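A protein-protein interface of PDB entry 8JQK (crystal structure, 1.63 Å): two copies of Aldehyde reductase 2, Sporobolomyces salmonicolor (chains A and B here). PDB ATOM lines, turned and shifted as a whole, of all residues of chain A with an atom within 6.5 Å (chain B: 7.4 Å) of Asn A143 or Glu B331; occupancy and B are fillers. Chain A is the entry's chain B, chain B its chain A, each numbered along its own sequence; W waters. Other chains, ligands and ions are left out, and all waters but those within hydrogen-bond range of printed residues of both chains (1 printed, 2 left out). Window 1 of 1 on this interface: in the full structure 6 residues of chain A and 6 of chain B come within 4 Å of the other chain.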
ATOM      1  N   LYS A 141     -11.225 -22.717  24.425  1.00  0.00           N
ATOM      2  CA  LYS A 141     -12.191 -21.739  23.942  1.00  0.00           C
ATOM      3  C   LYS A 141     -12.596 -22.169  22.542  1.00  0.00           C
ATOM      4  O   LYS A 141     -11.738 -22.203  21.634  1.00  0.00           O
ATOM      5  CB  LYS A 141     -11.601 -20.324  23.903  1.00  0.00           C
ATOM      6  CG  LYS A 141     -11.072 -19.769  25.215  1.00  0.00           C
ATOM      7  CD  LYS A 141     -12.062 -19.969  26.340  1.00  0.00           C
ATOM      8  CE  LYS A 141     -12.083 -18.774  27.280  1.00  0.00           C
ATOM      9  NZ  LYS A 141     -13.283 -18.800  28.166  1.00  0.00           N
ATOM     10  N   PRO A 142     -13.860 -22.501  22.309  1.00  0.00           N
ATOM     11  CA  PRO A 142     -14.249 -22.984  20.985  1.00  0.00           C
ATOM     12  C   PRO A 142     -14.186 -21.853  19.976  1.00  0.00           C
ATOM     13  O   PRO A 142     -14.439 -20.689  20.299  1.00  0.00           O
ATOM     14  CB  PRO A 142     -15.693 -23.467  21.185  1.00  0.00           C
ATOM     15  CG  PRO A 142     -15.899 -23.521  22.674  1.00  0.00           C
ATOM     16  CD  PRO A 142     -14.994 -22.484  23.246  1.00  0.00           C
ATOM     17  N   ASN A 143     -13.847 -22.213  18.740  1.00  0.00           N
ATOM     18  CA  ASN A 143     -13.899 -21.295  17.606  1.00  0.00           C
ATOM     19  C   ASN A 143     -13.095 -20.023  17.869  1.00  0.00           C
ATOM     20  O   ASN A 143     -13.597 -18.902  17.759  1.00  0.00           O
ATOM     21  CB  ASN A 143     -15.350 -20.976  17.257  1.00  0.00           C
ATOM     22  CG  ASN A 143     -16.234 -22.201  17.309  1.00  0.00           C
ATOM     23  OD1 ASN A 143     -16.970 -22.410  18.273  1.00  0.00           O
ATOM     24  ND2 ASN A 143     -16.175 -23.017  16.265  1.00  0.00           N
ATOM     25  N   VAL A 144     -11.838 -20.210  18.257  1.00  0.00           N
ATOM     26  CA  VAL A 144     -10.854 -19.136  18.335  1.00  0.00           C
ATOM     27  C   VAL A 144      -9.672 -19.543  17.462  1.00  0.00           C
ATOM     28  O   VAL A 144      -8.994 -20.537  17.750  1.00  0.00           O
ATOM     29  CB  VAL A 144     -10.416 -18.850  19.780  1.00  0.00           C
ATOM     30  CG1 VAL A 144      -9.457 -17.686  19.813  1.00  0.00           C
ATOM     31  CG2 VAL A 144     -11.629 -18.545  20.652  1.00  0.00           C
ATOM     32  N   GLU A 145      -9.434 -18.778  16.399  1.00  0.00           N
ATOM     33  CA  GLU A 145      -8.400 -19.078  15.423  1.00  0.00           C
ATOM     34  C   GLU A 145      -7.036 -18.601  15.912  1.00  0.00           C
ATOM     35  O   GLU A 145      -6.923 -17.758  16.807  1.00  0.00           O
ATOM     36  CB  GLU A 145      -8.735 -18.411  14.085  1.00  0.00           C
ATOM     37  CG  GLU A 145      -9.037 -19.360  12.932  1.00  0.00           C
ATOM     38  CD  GLU A 145      -9.291 -18.618  11.629  1.00  0.00           C
ATOM     39  OE1 GLU A 145      -8.997 -17.405  11.567  1.00  0.00           O
ATOM     40  OE2 GLU A 145      -9.816 -19.237  10.678  1.00  0.00           O
ATOM     41  N   GLY A 146      -5.990 -19.160  15.309  1.00  0.00           N
ATOM     42  CA  GLY A 146      -4.641 -18.689  15.559  1.00  0.00           C
ATOM     43  C   GLY A 146      -4.086 -18.987  16.933  1.00  0.00           C
ATOM     44  O   GLY A 146      -3.258 -18.221  17.438  1.00  0.00           O
ATOM     45  N   ASP A 302     -24.601 -28.101  20.025  1.00  0.00           N
ATOM     46  CA  ASP A 302     -23.213 -27.903  19.537  1.00  0.00           C
ATOM     47  C   ASP A 302     -22.445 -27.010  20.515  1.00  0.00           C
ATOM     48  O   ASP A 302     -23.001 -25.991  20.957  1.00  0.00           O
ATOM     49  CB  ASP A 302     -23.250 -27.307  18.127  1.00  0.00           C
ATOM     50  CG  ASP A 302     -22.020 -26.515  17.723  1.00  0.00           C
ATOM     51  OD1 ASP A 302     -21.010 -27.149  17.380  1.00  0.00           O
ATOM     52  OD2 ASP A 302     -22.095 -25.271  17.735  1.00  0.00           O
ATOM     53  N   GLN A 303     -21.222 -27.422  20.857  1.00  0.00           N
ATOM     54  CA  GLN A 303     -20.354 -26.627  21.764  1.00  0.00           C
ATOM     55  C   GLN A 303     -19.295 -25.901  20.930  1.00  0.00           C
ATOM     56  O   GLN A 303     -18.404 -25.297  21.530  1.00  0.00           O
ATOM     57  CB  GLN A 303     -19.717 -27.539  22.809  1.00  0.00           C
ATOM     58  CG  GLN A 303     -20.269 -28.957  22.804  1.00  0.00           C
ATOM     59  CD  GLN A 303     -19.884 -29.728  24.043  1.00  0.00           C
ATOM     60  OE1 GLN A 303     -18.709 -29.848  24.384  1.00  0.00           O
ATOM     61  NE2 GLN A 303     -20.882 -30.255  24.730  1.00  0.00           N
ATOM     62  N   GLY A 304     -19.395 -25.978  19.605  1.00  0.00           N
ATOM     63  CA  GLY A 304     -18.347 -25.406  18.742  1.00  0.00           C
ATOM     64  C   GLY A 304     -17.184 -26.364  18.541  1.00  0.00           C
ATOM     65  O   GLY A 304     -17.338 -27.549  18.846  1.00  0.00           O
ATOM     66  N   GLN A 305     -16.082 -25.873  17.975  1.00  0.00           N
ATOM     67  CA  GLN A 305     -14.916 -26.739  17.675  1.00  0.00           C
ATOM     68  C   GLN A 305     -13.635 -26.130  18.244  1.00  0.00           C
ATOM     69  O   GLN A 305     -13.504 -24.903  18.209  1.00  0.00           O
ATOM     70  CB  GLN A 305     -14.743 -26.863  16.163  1.00  0.00           C
ATOM     71  CG  GLN A 305     -15.357 -28.114  15.557  1.00  0.00           C
ATOM     72  CD  GLN A 305     -14.708 -28.442  14.235  1.00  0.00           C
ATOM     73  OE1 GLN A 305     -14.397 -29.595  13.944  1.00  0.00           O
ATOM     74  NE2 GLN A 305     -14.487 -27.421  13.423  1.00  0.00           N
ATOM     75  N   ASP A 306     -12.717 -26.973  18.710  1.00  0.00           N
ATOM     76  CA  ASP A 306     -11.429 -26.505  19.205  1.00  0.00           C
ATOM     77  C   ASP A 306     -10.457 -26.409  18.035  1.00  0.00           C
ATOM     78  O   ASP A 306     -10.074 -27.425  17.447  1.00  0.00           O
ATOM     79  CB  ASP A 306     -10.939 -27.462  20.292  1.00  0.00           C
ATOM     80  CG  ASP A 306      -9.619 -27.051  20.899  1.00  0.00           C
ATOM     81  OD1 ASP A 306      -9.154 -25.928  20.629  1.00  0.00           O
ATOM     82  OD2 ASP A 306      -9.066 -27.854  21.681  1.00  0.00           O
ATOM     83  N   LEU A 307     -10.071 -25.181  17.691  1.00  0.00           N
ATOM     84  CA  LEU A 307      -9.157 -24.915  16.592  1.00  0.00           C
ATOM     85  C   LEU A 307      -7.718 -24.755  17.052  1.00  0.00           C
ATOM     86  O   LEU A 307      -6.844 -24.484  16.225  1.00  0.00           O
ATOM     87  CB  LEU A 307      -9.591 -23.657  15.831  1.00  0.00           C
ATOM     88  CG  LEU A 307     -10.921 -23.718  15.077  1.00  0.00           C
ATOM     89  CD1 LEU A 307     -11.504 -22.319  14.904  1.00  0.00           C
ATOM     90  CD2 LEU A 307     -10.742 -24.405  13.731  1.00  0.00           C
ATOM     91  N   ILE B 210     -24.487  -9.001  14.991  1.00  0.00           N
ATOM     92  CA  ILE B 210     -23.090  -8.665  14.720  1.00  0.00           C
ATOM     93  C   ILE B 210     -22.680  -9.296  13.396  1.00  0.00           C
ATOM     94  O   ILE B 210     -22.751 -10.522  13.236  1.00  0.00           O
ATOM     95  CB  ILE B 210     -22.160  -9.136  15.849  1.00  0.00           C
ATOM     96  CG1 ILE B 210     -22.672  -8.677  17.216  1.00  0.00           C
ATOM     97  CG2 ILE B 210     -20.726  -8.668  15.605  1.00  0.00           C
ATOM     98  CD1 ILE B 210     -21.801  -9.142  18.361  1.00  0.00           C
ATOM     99  N   TYR B 247     -25.770 -11.894  21.714  1.00  0.00           N
ATOM    100  CA  TYR B 247     -25.377 -11.544  20.358  1.00  0.00           C
ATOM    101  C   TYR B 247     -25.956 -12.576  19.394  1.00  0.00           C
ATOM    102  O   TYR B 247     -26.354 -13.675  19.796  1.00  0.00           O
ATOM    103  CB  TYR B 247     -23.851 -11.511  20.206  1.00  0.00           C
ATOM    104  CG  TYR B 247     -23.296 -12.883  19.899  1.00  0.00           C
ATOM    105  CD1 TYR B 247     -23.108 -13.815  20.905  1.00  0.00           C
ATOM    106  CD2 TYR B 247     -23.000 -13.259  18.590  1.00  0.00           C
ATOM    107  CE1 TYR B 247     -22.630 -15.079  20.626  1.00  0.00           C
ATOM    108  CE2 TYR B 247     -22.527 -14.520  18.299  1.00  0.00           C
ATOM    109  CZ  TYR B 247     -22.340 -15.423  19.322  1.00  0.00           C
ATOM    110  OH  TYR B 247     -21.867 -16.683  19.035  1.00  0.00           O
ATOM    111  N   ALA B 285     -12.119  -7.122  24.265  1.00  0.00           N
ATOM    112  CA  ALA B 285     -11.105  -8.169  24.306  1.00  0.00           C
ATOM    113  C   ALA B 285     -10.912  -8.796  22.932  1.00  0.00           C
ATOM    114  O   ALA B 285      -9.778  -9.062  22.517  1.00  0.00           O
ATOM    115  CB  ALA B 285     -11.485  -9.232  25.337  1.00  0.00           C
ATOM    116  N   THR B 286     -12.011  -9.035  22.208  1.00  0.00           N
ATOM    117  CA  THR B 286     -11.902  -9.578  20.857  1.00  0.00           C
ATOM    118  C   THR B 286     -11.239  -8.586  19.910  1.00  0.00           C
ATOM    119  O   THR B 286     -10.411  -8.981  19.082  1.00  0.00           O
ATOM    120  CB  THR B 286     -13.280  -9.979  20.330  1.00  0.00           C
ATOM    121  OG1 THR B 286     -13.991 -10.714  21.336  1.00  0.00           O
ATOM    122  CG2 THR B 286     -13.148 -10.829  19.068  1.00  0.00           C
ATOM    123  N   LYS B 289      -7.430  -8.664  20.451  1.00  0.00           N
ATOM    124  CA  LYS B 289      -6.781  -9.847  19.902  1.00  0.00           C
ATOM    125  C   LYS B 289      -6.715  -9.781  18.381  1.00  0.00           C
ATOM    126  O   LYS B 289      -5.703 -10.164  17.781  1.00  0.00           O
ATOM    127  CB  LYS B 289      -7.519 -11.103  20.354  1.00  0.00           C
ATOM    128  CG  LYS B 289      -7.225 -12.314  19.501  1.00  0.00           C
ATOM    129  CD  LYS B 289      -7.628 -13.594  20.185  1.00  0.00           C
ATOM    130  CE  LYS B 289      -7.764 -14.710  19.166  1.00  0.00           C
ATOM    131  NZ  LYS B 289      -7.876 -14.182  17.777  1.00  0.00           N
ATOM    132  N   LEU B 290      -7.778  -9.292  17.739  1.00  0.00           N
ATOM    133  CA  LEU B 290      -7.787  -9.223  16.283  1.00  0.00           C
ATOM    134  C   LEU B 290      -6.831  -8.154  15.765  1.00  0.00           C
ATOM    135  O   LEU B 290      -6.314  -8.279  14.649  1.00  0.00           O
ATOM    136  CB  LEU B 290      -9.208  -8.971  15.779  1.00  0.00           C
ATOM    137  CG  LEU B 290     -10.197 -10.112  16.041  1.00  0.00           C
ATOM    138  CD1 LEU B 290     -11.609  -9.726  15.621  1.00  0.00           C
ATOM    139  CD2 LEU B 290      -9.759 -11.385  15.331  1.00  0.00           C
ATOM    140  N   PRO B 325     -23.767 -26.255  11.637  1.00  0.00           N
ATOM    141  CA  PRO B 325     -23.668 -27.044  12.876  1.00  0.00           C
ATOM    142  C   PRO B 325     -24.333 -26.377  14.062  1.00  0.00           C
ATOM    143  O   PRO B 325     -24.647 -27.059  15.047  1.00  0.00           O
ATOM    144  CB  PRO B 325     -22.153 -27.169  13.097  1.00  0.00           C
ATOM    145  CG  PRO B 325     -21.561 -26.030  12.329  1.00  0.00           C
ATOM    146  CD  PRO B 325     -22.447 -25.834  11.138  1.00  0.00           C
ATOM    147  N   TRP B 327     -24.880 -22.124  16.048  1.00  0.00           N
ATOM    148  CA  TRP B 327     -24.668 -20.684  16.000  1.00  0.00           C
ATOM    149  C   TRP B 327     -23.247 -20.373  15.553  1.00  0.00           C
ATOM    150  O   TRP B 327     -22.295 -21.074  15.910  1.00  0.00           O
ATOM    151  CB  TRP B 327     -24.903 -20.065  17.378  1.00  0.00           C
ATOM    152  CG  TRP B 327     -26.314 -20.131  17.893  1.00  0.00           C
ATOM    153  CD1 TRP B 327     -26.746 -20.826  18.984  1.00  0.00           C
ATOM    154  CD2 TRP B 327     -27.464 -19.444  17.375  1.00  0.00           C
ATOM    155  NE1 TRP B 327     -28.094 -20.638  19.165  1.00  0.00           N
ATOM    156  CE2 TRP B 327     -28.558 -19.788  18.196  1.00  0.00           C
ATOM    157  CE3 TRP B 327     -27.676 -18.577  16.300  1.00  0.00           C
ATOM    158  CZ2 TRP B 327     -29.848 -19.300  17.970  1.00  0.00           C
ATOM    159  CZ3 TRP B 327     -28.961 -18.093  16.078  1.00  0.00           C
ATOM    160  CH2 TRP B 327     -30.025 -18.455  16.908  1.00  0.00           C
ATOM    161  N   ARG B 328     -23.105 -19.322  14.754  1.00  0.00           N
ATOM    162  CA  ARG B 328     -21.785 -18.769  14.491  1.00  0.00           C
ATOM    163  C   ARG B 328     -21.260 -18.101  15.758  1.00  0.00           C
ATOM    164  O   ARG B 328     -22.021 -17.495  16.519  1.00  0.00           O
ATOM    165  CB  ARG B 328     -21.856 -17.774  13.333  1.00  0.00           C
ATOM    166  CG  ARG B 328     -20.520 -17.262  12.844  1.00  0.00           C
ATOM    167  CD  ARG B 328     -20.690 -16.517  11.526  1.00  0.00           C
ATOM    168  NE  ARG B 328     -19.423 -16.016  11.004  1.00  0.00           N
ATOM    169  CZ  ARG B 328     -18.624 -16.704  10.201  1.00  0.00           C
ATOM    170  NH1 ARG B 328     -18.867 -17.969   9.901  1.00  0.00           N
ATOM    171  NH2 ARG B 328     -17.540 -16.113   9.702  1.00  0.00           N
ATOM    172  N   SER B 329     -19.955 -18.235  15.995  1.00  0.00           N
ATOM    173  CA  SER B 329     -19.334 -17.772  17.231  1.00  0.00           C
ATOM    174  C   SER B 329     -19.199 -16.249  17.253  1.00  0.00           C
ATOM    175  O   SER B 329     -19.242 -15.582  16.218  1.00  0.00           O
ATOM    176  CB  SER B 329     -17.964 -18.423  17.404  1.00  0.00           C
ATOM    177  OG  SER B 329     -16.954 -17.643  16.790  1.00  0.00           O
ATOM    178  N   ILE B 330     -19.046 -15.696  18.464  1.00  0.00           N
ATOM    179  CA  ILE B 330     -18.904 -14.244  18.580  1.00  0.00           C
ATOM    180  C   ILE B 330     -17.586 -13.772  17.977  1.00  0.00           C
ATOM    181  O   ILE B 330     -17.540 -12.718  17.329  1.00  0.00           O
ATOM    182  CB  ILE B 330     -19.065 -13.770  20.036  1.00  0.00           C
ATOM    183  CG1 ILE B 330     -19.331 -12.258  20.046  1.00  0.00           C
ATOM    184  CG2 ILE B 330     -17.842 -14.093  20.879  1.00  0.00           C
ATOM    185  CD1 ILE B 330     -20.053 -11.762  21.268  1.00  0.00           C
ATOM    186  N   GLU B 331     -16.495 -14.531  18.153  1.00  0.00           N
ATOM    187  CA  GLU B 331     -15.247 -14.085  17.541  1.00  0.00           C
ATOM    188  C   GLU B 331     -15.369 -14.109  16.026  1.00  0.00           C
ATOM    189  O   GLU B 331     -14.926 -13.177  15.343  1.00  0.00           O
ATOM    190  CB  GLU B 331     -14.050 -14.929  17.992  1.00  0.00           C
ATOM    191  CG  GLU B 331     -12.910 -14.882  16.965  1.00  0.00           C
ATOM    192  CD  GLU B 331     -11.546 -15.247  17.520  1.00  0.00           C
ATOM    193  OE1 GLU B 331     -11.083 -14.589  18.476  1.00  0.00           O
ATOM    194  OE2 GLU B 331     -10.923 -16.181  16.976  1.00  0.00           O
ATOM    195  N   GLU B 332     -16.001 -15.153  15.488  1.00  0.00           N
ATOM    196  CA  GLU B 332     -16.240 -15.199  14.053  1.00  0.00           C
ATOM    197  C   GLU B 332     -17.152 -14.056  13.617  1.00  0.00           C
ATOM    198  O   GLU B 332     -16.909 -13.422  12.584  1.00  0.00           O
ATOM    199  CB  GLU B 332     -16.840 -16.555  13.675  1.00  0.00           C
ATOM    200  CG  GLU B 332     -15.819 -17.686  13.645  1.00  0.00           C
ATOM    201  CD  GLU B 332     -15.973 -18.597  12.441  1.00  0.00           C
ATOM    202  OE1 GLU B 332     -16.608 -19.664  12.581  1.00  0.00           O
ATOM    203  OE2 GLU B 332     -15.455 -18.251  11.355  1.00  0.00           O
ATOM    204  N   SER B 333     -18.190 -13.761  14.407  1.00  0.00           N
ATOM    205  CA  SER B 333     -19.101 -12.671  14.063  1.00  0.00           C
ATOM    206  C   SER B 333     -18.411 -11.313  14.150  1.00  0.00           C
ATOM    207  O   SER B 333     -18.598 -10.458  13.274  1.00  0.00           O
ATOM    208  CB  SER B 333     -20.344 -12.709  14.958  1.00  0.00           C
ATOM    209  OG  SER B 333     -20.868 -14.026  15.061  1.00  0.00           O
ATOM    210  N   ILE B 334     -17.612 -11.090  15.196  1.00  0.00           N
ATOM    211  CA  ILE B 334     -16.893  -9.824  15.304  1.00  0.00           C
ATOM    212  C   ILE B 334     -15.862  -9.703  14.186  1.00  0.00           C
ATOM    213  O   ILE B 334     -15.648  -8.615  13.636  1.00  0.00           O
ATOM    214  CB  ILE B 334     -16.268  -9.683  16.703  1.00  0.00           C
ATOM    215  CG1 ILE B 334     -17.368  -9.442  17.739  1.00  0.00           C
ATOM    216  CG2 ILE B 334     -15.272  -8.533  16.752  1.00  0.00           C
ATOM    217  CD1 ILE B 334     -16.892  -9.548  19.177  1.00  0.00           C
ATOM    218  N   LYS B 335     -15.222 -10.817  13.819  1.00  0.00           N
ATOM    219  CA  LYS B 335     -14.292 -10.806  12.693  1.00  0.00           C
ATOM    220  C   LYS B 335     -15.005 -10.456  11.389  1.00  0.00           C
ATOM    221  O   LYS B 335     -14.449  -9.747  10.542  1.00  0.00           O
ATOM    222  CB  LYS B 335     -13.596 -12.163  12.580  1.00  0.00           C
ATOM    223  CG  LYS B 335     -12.223 -12.129  11.932  1.00  0.00           C
ATOM    224  CD  LYS B 335     -11.573 -13.508  11.976  1.00  0.00           C
ATOM    225  CE  LYS B 335     -10.144 -13.467  11.461  1.00  0.00           C
ATOM    226  NZ  LYS B 335      -9.881 -14.550  10.474  1.00  0.00           N
ATOM    227  N   ASP B 336     -16.238 -10.948  11.206  1.00  0.00           N
ATOM    228  CA  ASP B 336     -17.041 -10.537  10.059  1.00  0.00           C
ATOM    229  C   ASP B 336     -17.186  -9.021   9.993  1.00  0.00           C
ATOM    230  O   ASP B 336     -17.227  -8.441   8.902  1.00  0.00           O
ATOM    231  CB  ASP B 336     -18.435 -11.175  10.122  1.00  0.00           C
ATOM    232  CG  ASP B 336     -18.416 -12.673   9.875  1.00  0.00           C
ATOM    233  OD1 ASP B 336     -17.423 -13.185   9.319  1.00  0.00           O
ATOM    234  OD2 ASP B 336     -19.413 -13.340  10.225  1.00  0.00           O
ATOM    235  N   LEU B 337     -17.257  -8.368  11.153  1.00  0.00           N
ATOM    236  CA  LEU B 337     -17.506  -6.932  11.205  1.00  0.00           C
ATOM    237  C   LEU B 337     -16.235  -6.112  10.995  1.00  0.00           C
ATOM    238  O   LEU B 337     -16.211  -5.202  10.160  1.00  0.00           O
ATOM    239  CB  LEU B 337     -18.162  -6.569  12.538  1.00  0.00           C
ATOM    240  CG  LEU B 337     -18.407  -5.081  12.815  1.00  0.00           C
ATOM    241  CD1 LEU B 337     -19.399  -4.466  11.842  1.00  0.00           C
ATOM    242  CD2 LEU B 337     -18.894  -4.912  14.240  1.00  0.00           C
ATOM    243  N   VAL B 338     -15.179  -6.400  11.757  1.00  0.00           N
ATOM    244  CA  VAL B 338     -14.008  -5.527  11.813  1.00  0.00           C
ATOM    245  C   VAL B 338     -12.792  -6.104  11.107  1.00  0.00           C
ATOM    246  O   VAL B 338     -11.811  -5.368  10.901  1.00  0.00           O
ATOM    247  CB  VAL B 338     -13.633  -5.173  13.270  1.00  0.00           C
ATOM    248  CG1 VAL B 338     -14.827  -4.569  14.006  1.00  0.00           C
ATOM    249  CG2 VAL B 338     -13.097  -6.399  13.995  1.00  0.00           C
ATOM    250  N   GLY B 339     -12.816  -7.376  10.721  1.00  0.00           N
ATOM    251  CA  GLY B 339     -11.654  -8.001  10.118  1.00  0.00           C
ATOM    252  C   GLY B 339     -10.585  -8.360  11.139  1.00  0.00           C
ATOM    253  O   GLY B 339     -10.832  -8.467  12.346  1.00  0.00           O
HETATM  254  O   HOH W   1     -24.082 -23.176  18.569  1.00  0.00           O
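The side-chain carboxylate (OE2) of Glu B331 is in hydrogen-bond range of the backbone NH (N) of Glu A145, at 3.0 Å.
OE1 of Glu A145 lies within salt-bridge range of NZ of Lys B335.
Hydrophobic or aromatic side chains of chain A within 4 Å of the printed part of chain B: Val A144.
Among the printed residues, 8 pairs touch across the chains.
Among the printed residues, Asp or Glu carboxylates within 4 Å of a Lys or Arg side-chain nitrogen of the other chain: Glu A145 with Lys B335 (3.2 Å).
Asn A143 touches Ser B329 (CB to CB, 3.7 Å).
Glu B331 touches Asn A143.
Lys B289 touches Val A144 (CE to CG1, 3.5 Å).
OE2 of Glu B331 touches CA of Val A144 (3.3 Å).
NZ of Lys B289 touches O of Glu A145, at 3.8 Å.
Asp A302 touches Pro B325.
No position is printed for both chains.
The side-chain carboxylate (OE1) of Glu B331 lies within salt-bridge range of the side-chain amino group (NZ) of Lys B289, 3.3 Å away.
The backbone NH (N) of Glu B331 sits close to the side-chain hydroxyl (OG) of Ser B329 (3.4 Å).
N of Glu B332 sits at hydrogen-bond distance from OG of Ser B329, 3.0 Å away.
The side-chain hydroxyl (OG) of Ser B333 lies within hydrogen-bond range of the backbone carbonyl oxygen (O) of Ser B329.
The backbone NH (N) of Asn A143 lies within hydrogen-bond range of the backbone carbonyl oxygen (O) of Gln A305 (2.8 Å).
OD1 of Asp A302 lies within hydrogen-bond range of N of Gly A304, 3.0 Å away.
Asn A143 touches just these residues of chain B: Ser B329 and Glu B331.
Glu B331 touches three residues of chain A.
Of the printed residues of chain A, Pro B325 touches Asp A302.
Printed residues of chain A within 4 Å of Lys B335: Glu A145 (3.2 Å).
Of the printed residues of chain B, Val A144 touches Lys B289 and Glu B331.
Leu B290 touches none of the printed residues of chain A.
Gln A305 touches none of the printed residues of chain B.
Water W1 lies within hydrogen-bond range of N of Trp B327 (2.8 Å) and OD2 of Asp A302 (3.0 Å).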
